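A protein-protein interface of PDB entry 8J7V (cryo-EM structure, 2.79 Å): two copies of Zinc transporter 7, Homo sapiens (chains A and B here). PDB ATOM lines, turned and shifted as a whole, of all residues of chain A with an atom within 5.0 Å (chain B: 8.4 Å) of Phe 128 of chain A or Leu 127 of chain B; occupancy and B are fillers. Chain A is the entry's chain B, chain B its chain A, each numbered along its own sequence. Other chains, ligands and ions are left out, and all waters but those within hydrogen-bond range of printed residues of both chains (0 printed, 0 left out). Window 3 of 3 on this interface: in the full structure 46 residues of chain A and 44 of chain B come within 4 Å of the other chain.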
ATOM      1  N   PHE A  87      10.762  -8.395   7.585  1.00  0.00           N
ATOM      2  CA  PHE A  87      10.920  -8.654   6.161  1.00  0.00           C
ATOM      3  C   PHE A  87      10.465 -10.056   5.781  1.00  0.00           C
ATOM      4  O   PHE A  87      10.077 -10.273   4.634  1.00  0.00           O
ATOM      5  CB  PHE A  87      12.369  -8.415   5.734  1.00  0.00           C
ATOM      6  CG  PHE A  87      12.686  -6.969   5.470  1.00  0.00           C
ATOM      7  CD1 PHE A  87      12.047  -5.961   6.177  1.00  0.00           C
ATOM      8  CD2 PHE A  87      13.607  -6.614   4.504  1.00  0.00           C
ATOM      9  CE1 PHE A  87      12.330  -4.635   5.936  1.00  0.00           C
ATOM     10  CE2 PHE A  87      13.892  -5.285   4.258  1.00  0.00           C
ATOM     11  CZ  PHE A  87      13.254  -4.295   4.975  1.00  0.00           C
ATOM     12  N   VAL A 124      13.475  -9.891  -5.036  1.00  0.00           N
ATOM     13  CA  VAL A 124      13.445  -8.642  -4.287  1.00  0.00           C
ATOM     14  C   VAL A 124      13.630  -8.927  -2.810  1.00  0.00           C
ATOM     15  O   VAL A 124      14.419  -8.256  -2.129  1.00  0.00           O
ATOM     16  CB  VAL A 124      12.139  -7.877  -4.567  1.00  0.00           C
ATOM     17  CG1 VAL A 124      11.955  -6.752  -3.566  1.00  0.00           C
ATOM     18  CG2 VAL A 124      12.147  -7.333  -5.983  1.00  0.00           C
ATOM     19  N   ASN A 125      12.984  -9.992  -2.321  1.00  0.00           N
ATOM     20  CA  ASN A 125      13.110 -10.357  -0.916  1.00  0.00           C
ATOM     21  C   ASN A 125      14.572 -10.539  -0.551  1.00  0.00           C
ATOM     22  O   ASN A 125      15.073  -9.903   0.386  1.00  0.00           O
ATOM     23  CB  ASN A 125      12.316 -11.633  -0.634  1.00  0.00           C
ATOM     24  CG  ASN A 125      10.844 -11.363  -0.422  1.00  0.00           C
ATOM     25  OD1 ASN A 125       9.995 -12.183  -0.773  1.00  0.00           O
ATOM     26  ND2 ASN A 125      10.530 -10.210   0.155  1.00  0.00           N
ATOM     27  N   GLY A 126      15.294 -11.323  -1.357  1.00  0.00           N
ATOM     28  CA  GLY A 126      16.699 -11.553  -1.079  1.00  0.00           C
ATOM     29  C   GLY A 126      17.481 -10.260  -1.021  1.00  0.00           C
ATOM     30  O   GLY A 126      18.259 -10.037  -0.090  1.00  0.00           O
ATOM     31  N   LEU A 127      17.223  -9.357  -1.971  1.00  0.00           N
ATOM     32  CA  LEU A 127      17.913  -8.075  -1.963  1.00  0.00           C
ATOM     33  C   LEU A 127      17.595  -7.311  -0.690  1.00  0.00           C
ATOM     34  O   LEU A 127      18.500  -6.846   0.013  1.00  0.00           O
ATOM     35  CB  LEU A 127      17.528  -7.265  -3.198  1.00  0.00           C
ATOM     36  CG  LEU A 127      18.061  -7.819  -4.516  1.00  0.00           C
ATOM     37  CD1 LEU A 127      17.736  -6.871  -5.648  1.00  0.00           C
ATOM     38  CD2 LEU A 127      19.557  -8.059  -4.429  1.00  0.00           C
ATOM     39  N   PHE A 128      16.313  -7.249  -0.328  1.00  0.00           N
ATOM     40  CA  PHE A 128      15.956  -6.536   0.884  1.00  0.00           C
ATOM     41  C   PHE A 128      16.383  -7.300   2.124  1.00  0.00           C
ATOM     42  O   PHE A 128      16.468  -6.709   3.203  1.00  0.00           O
ATOM     43  CB  PHE A 128      14.458  -6.242   0.902  1.00  0.00           C
ATOM     44  CG  PHE A 128      14.083  -5.006   0.133  1.00  0.00           C
ATOM     45  CD1 PHE A 128      15.052  -4.076  -0.215  1.00  0.00           C
ATOM     46  CD2 PHE A 128      12.774  -4.773  -0.244  1.00  0.00           C
ATOM     47  CE1 PHE A 128      14.720  -2.940  -0.923  1.00  0.00           C
ATOM     48  CE2 PHE A 128      12.436  -3.635  -0.954  1.00  0.00           C
ATOM     49  CZ  PHE A 128      13.411  -2.720  -1.292  1.00  0.00           C
ATOM     50  N   LEU A 129      16.686  -8.589   1.989  1.00  0.00           N
ATOM     51  CA  LEU A 129      17.269  -9.318   3.100  1.00  0.00           C
ATOM     52  C   LEU A 129      18.780  -9.187   3.149  1.00  0.00           C
ATOM     53  O   LEU A 129      19.371  -9.410   4.210  1.00  0.00           O
ATOM     54  CB  LEU A 129      16.875 -10.795   3.033  1.00  0.00           C
ATOM     55  CG  LEU A 129      16.295 -11.379   4.321  1.00  0.00           C
ATOM     56  CD1 LEU A 129      15.482 -10.341   5.077  1.00  0.00           C
ATOM     57  CD2 LEU A 129      15.435 -12.576   3.997  1.00  0.00           C
ATOM     58  N   ILE A 130      19.417  -8.818   2.041  1.00  0.00           N
ATOM     59  CA  ILE A 130      20.867  -8.691   2.050  1.00  0.00           C
ATOM     60  C   ILE A 130      21.299  -7.270   2.400  1.00  0.00           C
ATOM     61  O   ILE A 130      22.339  -7.083   3.041  1.00  0.00           O
ATOM     62  CB  ILE A 130      21.449  -9.158   0.702  1.00  0.00           C
ATOM     63  CG1 ILE A 130      22.114 -10.525   0.871  1.00  0.00           C
ATOM     64  CG2 ILE A 130      22.430  -8.148   0.109  1.00  0.00           C
ATOM     65  CD1 ILE A 130      22.535 -11.162  -0.426  1.00  0.00           C
ATOM     66  N   PHE A 131      20.509  -6.268   2.022  1.00  0.00           N
ATOM     67  CA  PHE A 131      20.832  -4.883   2.335  1.00  0.00           C
ATOM     68  C   PHE A 131      20.824  -4.670   3.843  1.00  0.00           C
ATOM     69  O   PHE A 131      21.877  -4.425   4.444  1.00  0.00           O
ATOM     70  CB  PHE A 131      19.841  -3.933   1.657  1.00  0.00           C
ATOM     71  CG  PHE A 131      19.949  -3.903   0.153  1.00  0.00           C
ATOM     72  CD1 PHE A 131      21.017  -4.499  -0.500  1.00  0.00           C
ATOM     73  CD2 PHE A 131      18.973  -3.282  -0.607  1.00  0.00           C
ATOM     74  CE1 PHE A 131      21.108  -4.472  -1.879  1.00  0.00           C
ATOM     75  CE2 PHE A 131      19.060  -3.253  -1.986  1.00  0.00           C
ATOM     76  CZ  PHE A 131      20.128  -3.848  -2.622  1.00  0.00           C
ATOM     77  N   THR A 132      19.645  -4.825   4.454  1.00  0.00           N
ATOM     78  CA  THR A 132      19.466  -4.512   5.870  1.00  0.00           C
ATOM     79  C   THR A 132      20.440  -5.288   6.745  1.00  0.00           C
ATOM     80  O   THR A 132      21.094  -4.714   7.624  1.00  0.00           O
ATOM     81  CB  THR A 132      18.030  -4.811   6.296  1.00  0.00           C
ATOM     82  OG1 THR A 132      17.823  -6.229   6.312  1.00  0.00           O
ATOM     83  CG2 THR A 132      17.054  -4.177   5.331  1.00  0.00           C
ATOM     84  N   LEU B 120      20.168  -6.789 -14.562  1.00  0.00           N
ATOM     85  CA  LEU B 120      20.145  -7.087 -13.135  1.00  0.00           C
ATOM     86  C   LEU B 120      20.837  -5.998 -12.332  1.00  0.00           C
ATOM     87  O   LEU B 120      20.340  -5.589 -11.276  1.00  0.00           O
ATOM     88  CB  LEU B 120      20.800  -8.442 -12.870  1.00  0.00           C
ATOM     89  CG  LEU B 120      19.905  -9.675 -12.996  1.00  0.00           C
ATOM     90  CD1 LEU B 120      20.612 -10.903 -12.459  1.00  0.00           C
ATOM     91  CD2 LEU B 120      18.586  -9.458 -12.277  1.00  0.00           C
ATOM     92  N   ALA B 121      21.964  -5.486 -12.838  1.00  0.00           N
ATOM     93  CA  ALA B 121      22.643  -4.393 -12.155  1.00  0.00           C
ATOM     94  C   ALA B 121      21.720  -3.193 -12.017  1.00  0.00           C
ATOM     95  O   ALA B 121      21.516  -2.675 -10.912  1.00  0.00           O
ATOM     96  CB  ALA B 121      23.916  -4.010 -12.905  1.00  0.00           C
ATOM     97  N   GLY B 122      21.095  -2.786 -13.124  1.00  0.00           N
ATOM     98  CA  GLY B 122      20.150  -1.686 -13.067  1.00  0.00           C
ATOM     99  C   GLY B 122      18.969  -1.979 -12.168  1.00  0.00           C
ATOM    100  O   GLY B 122      18.348  -1.059 -11.633  1.00  0.00           O
ATOM    101  N   PHE B 123      18.641  -3.260 -11.986  1.00  0.00           N
ATOM    102  CA  PHE B 123      17.606  -3.594 -11.021  1.00  0.00           C
ATOM    103  C   PHE B 123      18.121  -3.481  -9.595  1.00  0.00           C
ATOM    104  O   PHE B 123      17.415  -2.972  -8.719  1.00  0.00           O
ATOM    105  CB  PHE B 123      17.062  -4.995 -11.280  1.00  0.00           C
ATOM    106  CG  PHE B 123      15.807  -5.294 -10.523  1.00  0.00           C
ATOM    107  CD1 PHE B 123      14.747  -4.407 -10.546  1.00  0.00           C
ATOM    108  CD2 PHE B 123      15.687  -6.450  -9.780  1.00  0.00           C
ATOM    109  CE1 PHE B 123      13.596  -4.671  -9.848  1.00  0.00           C
ATOM    110  CE2 PHE B 123      14.533  -6.719  -9.081  1.00  0.00           C
ATOM    111  CZ  PHE B 123      13.487  -5.828  -9.116  1.00  0.00           C
ATOM    112  N   VAL B 124      19.344  -3.950  -9.338  1.00  0.00           N
ATOM    113  CA  VAL B 124      19.859  -3.937  -7.972  1.00  0.00           C
ATOM    114  C   VAL B 124      20.151  -2.509  -7.532  1.00  0.00           C
ATOM    115  O   VAL B 124      19.708  -2.071  -6.462  1.00  0.00           O
ATOM    116  CB  VAL B 124      21.104  -4.834  -7.857  1.00  0.00           C
ATOM    117  CG1 VAL B 124      21.870  -4.519  -6.587  1.00  0.00           C
ATOM    118  CG2 VAL B 124      20.706  -6.297  -7.890  1.00  0.00           C
ATOM    119  N   ASN B 125      20.865  -1.754  -8.373  1.00  0.00           N
ATOM    120  CA  ASN B 125      21.278  -0.399  -8.017  1.00  0.00           C
ATOM    121  C   ASN B 125      20.077   0.472  -7.683  1.00  0.00           C
ATOM    122  O   ASN B 125      20.046   1.129  -6.636  1.00  0.00           O
ATOM    123  CB  ASN B 125      22.086   0.214  -9.159  1.00  0.00           C
ATOM    124  CG  ASN B 125      23.577   0.122  -8.931  1.00  0.00           C
ATOM    125  OD1 ASN B 125      24.115   0.743  -8.015  1.00  0.00           O
ATOM    126  ND2 ASN B 125      24.255  -0.658  -9.762  1.00  0.00           N
ATOM    127  N   GLY B 126      19.063   0.462  -8.552  1.00  0.00           N
ATOM    128  CA  GLY B 126      17.830   1.163  -8.236  1.00  0.00           C
ATOM    129  C   GLY B 126      17.212   0.671  -6.943  1.00  0.00           C
ATOM    130  O   GLY B 126      16.852   1.468  -6.072  1.00  0.00           O
ATOM    131  N   LEU B 127      17.136  -0.653  -6.777  1.00  0.00           N
ATOM    132  CA  LEU B 127      16.603  -1.203  -5.535  1.00  0.00           C
ATOM    133  C   LEU B 127      17.490  -0.855  -4.353  1.00  0.00           C
ATOM    134  O   LEU B 127      17.017  -0.822  -3.212  1.00  0.00           O
ATOM    135  CB  LEU B 127      16.436  -2.719  -5.647  1.00  0.00           C
ATOM    136  CG  LEU B 127      15.168  -3.231  -6.333  1.00  0.00           C
ATOM    137  CD1 LEU B 127      14.853  -4.640  -5.868  1.00  0.00           C
ATOM    138  CD2 LEU B 127      13.985  -2.312  -6.077  1.00  0.00           C
ATOM    139  N   PHE B 128      18.774  -0.598  -4.601  1.00  0.00           N
ATOM    140  CA  PHE B 128      19.627  -0.069  -3.545  1.00  0.00           C
ATOM    141  C   PHE B 128      19.226   1.356  -3.201  1.00  0.00           C
ATOM    142  O   PHE B 128      19.033   1.694  -2.026  1.00  0.00           O
ATOM    143  CB  PHE B 128      21.090  -0.131  -3.975  1.00  0.00           C
ATOM    144  CG  PHE B 128      22.061  -0.056  -2.835  1.00  0.00           C
ATOM    145  CD1 PHE B 128      22.206  -1.119  -1.961  1.00  0.00           C
ATOM    146  CD2 PHE B 128      22.832   1.077  -2.641  1.00  0.00           C
ATOM    147  CE1 PHE B 128      23.101  -1.053  -0.911  1.00  0.00           C
ATOM    148  CE2 PHE B 128      23.726   1.150  -1.594  1.00  0.00           C
ATOM    149  CZ  PHE B 128      23.862   0.083  -0.727  1.00  0.00           C
ATOM    150  N   LEU B 129      19.047   2.194  -4.225  1.00  0.00           N
ATOM    151  CA  LEU B 129      18.860   3.621  -3.994  1.00  0.00           C
ATOM    152  C   LEU B 129      17.541   3.919  -3.304  1.00  0.00           C
ATOM    153  O   LEU B 129      17.438   4.914  -2.579  1.00  0.00           O
ATOM    154  CB  LEU B 129      18.952   4.376  -5.315  1.00  0.00           C
ATOM    155  CG  LEU B 129      20.368   4.501  -5.866  1.00  0.00           C
ATOM    156  CD1 LEU B 129      20.350   5.268  -7.164  1.00  0.00           C
ATOM    157  CD2 LEU B 129      21.260   5.185  -4.847  1.00  0.00           C
ATOM    158  N   ILE B 130      16.524   3.087  -3.524  1.00  0.00           N
ATOM    159  CA  ILE B 130      15.287   3.221  -2.761  1.00  0.00           C
ATOM    160  C   ILE B 130      15.552   2.951  -1.287  1.00  0.00           C
ATOM    161  O   ILE B 130      15.149   3.730  -0.414  1.00  0.00           O
ATOM    162  CB  ILE B 130      14.202   2.287  -3.326  1.00  0.00           C
ATOM    163  CG1 ILE B 130      13.499   2.952  -4.508  1.00  0.00           C
ATOM    164  CG2 ILE B 130      13.193   1.915  -2.252  1.00  0.00           C
ATOM    165  CD1 ILE B 130      12.267   2.219  -4.970  1.00  0.00           C
ATOM    166  N   PHE B 131      16.280   1.868  -0.995  1.00  0.00           N
ATOM    167  CA  PHE B 131      16.485   1.450   0.389  1.00  0.00           C
ATOM    168  C   PHE B 131      17.183   2.538   1.193  1.00  0.00           C
ATOM    169  O   PHE B 131      16.663   2.998   2.220  1.00  0.00           O
ATOM    170  CB  PHE B 131      17.279   0.143   0.418  1.00  0.00           C
ATOM    171  CG  PHE B 131      17.938  -0.146   1.736  1.00  0.00           C
ATOM    172  CD1 PHE B 131      17.224  -0.721   2.769  1.00  0.00           C
ATOM    173  CD2 PHE B 131      19.285   0.125   1.928  1.00  0.00           C
ATOM    174  CE1 PHE B 131      17.832  -0.995   3.979  1.00  0.00           C
ATOM    175  CE2 PHE B 131      19.896  -0.147   3.134  1.00  0.00           C
ATOM    176  CZ  PHE B 131      19.170  -0.710   4.160  1.00  0.00           C
ATOM    177  N   THR B 132      18.333   3.011   0.700  1.00  0.00           N
ATOM    178  CA  THR B 132      19.021   4.121   1.349  1.00  0.00           C
ATOM    179  C   THR B 132      18.107   5.329   1.473  1.00  0.00           C
ATOM    180  O   THR B 132      18.107   6.010   2.507  1.00  0.00           O
ATOM    181  CB  THR B 132      20.287   4.488   0.576  1.00  0.00           C
ATOM    182  OG1 THR B 132      19.941   5.291  -0.559  1.00  0.00           O
ATOM    183  CG2 THR B 132      21.007   3.236   0.108  1.00  0.00           C
ATOM    184  N   ALA B 133      17.287   5.577   0.444  1.00  0.00           N
ATOM    185  CA  ALA B 133      16.323   6.670   0.494  1.00  0.00           C
ATOM    186  C   ALA B 133      15.478   6.578   1.751  1.00  0.00           C
ATOM    187  O   ALA B 133      15.417   7.529   2.541  1.00  0.00           O
ATOM    188  CB  ALA B 133      15.432   6.646  -0.747  1.00  0.00           C
ATOM    189  N   PHE B 134      14.898   5.398   1.997  1.00  0.00           N
ATOM    190  CA  PHE B 134      14.072   5.222   3.183  1.00  0.00           C
ATOM    191  C   PHE B 134      14.875   5.516   4.439  1.00  0.00           C
ATOM    192  O   PHE B 134      14.404   6.230   5.333  1.00  0.00           O
ATOM    193  CB  PHE B 134      13.505   3.803   3.227  1.00  0.00           C
ATOM    194  CG  PHE B 134      12.332   3.590   2.314  1.00  0.00           C
ATOM    195  CD1 PHE B 134      11.641   4.670   1.786  1.00  0.00           C
ATOM    196  CD2 PHE B 134      11.918   2.311   1.983  1.00  0.00           C
ATOM    197  CE1 PHE B 134      10.561   4.477   0.946  1.00  0.00           C
ATOM    198  CE2 PHE B 134      10.838   2.110   1.143  1.00  0.00           C
ATOM    199  CZ  PHE B 134      10.159   3.196   0.624  1.00  0.00           C
ATOM    200  N   GLY B 250      22.345   3.153 -13.648  1.00  0.00           N
ATOM    201  CA  GLY B 250      22.289   2.900 -12.218  1.00  0.00           C
ATOM    202  C   GLY B 250      23.444   3.531 -11.465  1.00  0.00           C
ATOM    203  O   GLY B 250      23.262   4.081 -10.377  1.00  0.00           O
ATOM    204  N   VAL B 296      15.053   7.448  -9.312  1.00  0.00           N
ATOM    205  CA  VAL B 296      15.238   6.033  -9.648  1.00  0.00           C
ATOM    206  C   VAL B 296      13.987   5.346 -10.171  1.00  0.00           C
ATOM    207  O   VAL B 296      14.074   4.183 -10.584  1.00  0.00           O
ATOM    208  CB  VAL B 296      15.763   5.213  -8.455  1.00  0.00           C
ATOM    209  CG1 VAL B 296      16.853   5.967  -7.749  1.00  0.00           C
ATOM    210  CG2 VAL B 296      14.636   4.899  -7.488  1.00  0.00           C
ATOM    211  N   LEU B 299      14.372   3.996 -14.126  1.00  0.00           N
ATOM    212  CA  LEU B 299      15.280   2.865 -14.277  1.00  0.00           C
ATOM    213  C   LEU B 299      14.665   1.588 -13.733  1.00  0.00           C
ATOM    214  O   LEU B 299      14.768   0.530 -14.363  1.00  0.00           O
ATOM    215  CB  LEU B 299      16.605   3.158 -13.573  1.00  0.00           C
ATOM    216  CG  LEU B 299      17.541   1.974 -13.330  1.00  0.00           C
ATOM    217  CD1 LEU B 299      18.388   1.698 -14.560  1.00  0.00           C
ATOM    218  CD2 LEU B 299      18.419   2.227 -12.118  1.00  0.00           C
ATOM    219  N   LEU B 300      14.010   1.671 -12.577  1.00  0.00           N
ATOM    220  CA  LEU B 300      13.304   0.530 -12.016  1.00  0.00           C
ATOM    221  C   LEU B 300      12.149   0.068 -12.886  1.00  0.00           C
ATOM    222  O   LEU B 300      11.966  -1.141 -13.038  1.00  0.00           O
ATOM    223  CB  LEU B 300      12.784   0.861 -10.619  1.00  0.00           C
ATOM    224  CG  LEU B 300      13.746   0.581  -9.468  1.00  0.00           C
ATOM    225  CD1 LEU B 300      12.997   0.610  -8.158  1.00  0.00           C
ATOM    226  CD2 LEU B 300      14.441  -0.757  -9.661  1.00  0.00           C
ATOM    227  N   SER B 303      13.762  -1.747 -15.881  1.00  0.00           N
ATOM    228  CA  SER B 303      14.364  -3.013 -15.472  1.00  0.00           C
ATOM    229  C   SER B 303      13.306  -4.057 -15.137  1.00  0.00           C
ATOM    230  O   SER B 303      13.451  -5.232 -15.497  1.00  0.00           O
ATOM    231  CB  SER B 303      15.290  -2.787 -14.279  1.00  0.00           C
ATOM    232  OG  SER B 303      16.025  -1.590 -14.433  1.00  0.00           O
ATOM    233  N   VAL B 304      12.243  -3.651 -14.439  1.00  0.00           N
ATOM    234  CA  VAL B 304      11.158  -4.573 -14.123  1.00  0.00           C
ATOM    235  C   VAL B 304      10.477  -5.043 -15.399  1.00  0.00           C
ATOM    236  O   VAL B 304      10.157  -6.227 -15.546  1.00  0.00           O
ATOM    237  CB  VAL B 304      10.164  -3.913 -13.151  1.00  0.00           C
ATOM    238  CG1 VAL B 304       8.844  -4.659 -13.136  1.00  0.00           C
ATOM    239  CG2 VAL B 304      10.750  -3.863 -11.757  1.00  0.00           C
ATOM    240  N   LEU B 307      12.837  -7.622 -17.083  1.00  0.00           N
ATOM    241  CA  LEU B 307      12.915  -8.888 -16.364  1.00  0.00           C
ATOM    242  C   LEU B 307      11.581  -9.624 -16.309  1.00  0.00           C
ATOM    243  O   LEU B 307      11.570 -10.831 -16.049  1.00  0.00           O
ATOM    244  CB  LEU B 307      13.440  -8.659 -14.948  1.00  0.00           C
ATOM    245  CG  LEU B 307      14.913  -8.264 -14.844  1.00  0.00           C
ATOM    246  CD1 LEU B 307      15.291  -7.971 -13.405  1.00  0.00           C
ATOM    247  CD2 LEU B 307      15.794  -9.354 -15.421  1.00  0.00           C
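Of the printed residues of chain B, Phe 128 of chain A touches Leu 127. Leu 127 of chain B touches just these residues of chain A: Val 124 (3.8 Å), Leu 127 (3.7 Å), Phe 128 (3.9 Å) and Phe 131 (3.4 Å). Printed residues of chain A within 4 Å of Phe 128 of chain B: Phe 131 (3.5 Å). Of the printed residues of chain B, Leu 127 of chain A touches Val 124 (3.8 Å) and Leu 127 (3.7 Å). Printed residues of chain B within 4 Å of Thr 132 of chain A: Phe 131. Of the printed residues of chain A, Phe 131 of chain B touches Phe 131 (3.96 Å) and Thr 132 (3.5 Å). The nearest printed residue of chain B that does not touch Leu 127 of chain A is Phe 123 of chain B (4.6 Å).
Hydrophobic or aromatic side chains of chain B that line the printed part of chain A: Phe 123, Val 124, Leu 127, Phe 128 and Phe 131.
Val 124 of chain A touches Leu 127 of chain B, and with the chains exchanged Leu 127 of chain A touches Val 124 of chain B. Leu 127 of chain B touches its own counterpart, Leu 127 of chain A. Phe 128 of chain A touches Leu 127 of chain B, but with the chains exchanged Leu 127 of chain A does not touch Phe 128 of chain B (6.4 Å). Phe 131 of chain A touches Leu 127 of chain B, but with the chains exchanged Leu 127 of chain A does not touch Phe 131 of chain B (6.8 Å). Positions printed for both chains: 124, 125, 126, 127, 128, 129, 130, 131 and 132.
O of Phe 128 of chain A lies close to OG1 of Thr 132 of chain A, 3.4 Å away.
Among the printed residues, merely in contact across the chains: Val 124 of chain A with Phe 123 of chain B (3.7 Å), Val 124 of chain A with Leu 127 of chain B (3.8 Å), Leu 127 of chain A with Val 124 of chain B (3.8 Å), Leu 127 of chain A with Leu 127 of chain B (3.7 Å), Phe 128 of chain A with Leu 127 of chain B (3.9 Å), Phe 131 of chain A with Leu 127 of chain B (3.4 Å), Phe 131 of chain A with Phe 128 of chain B (3.5 Å), Phe 131 of chain A with Phe 131 of chain B (3.96 Å) and Thr 132 of chain A with Phe 131 of chain B (3.5 Å).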
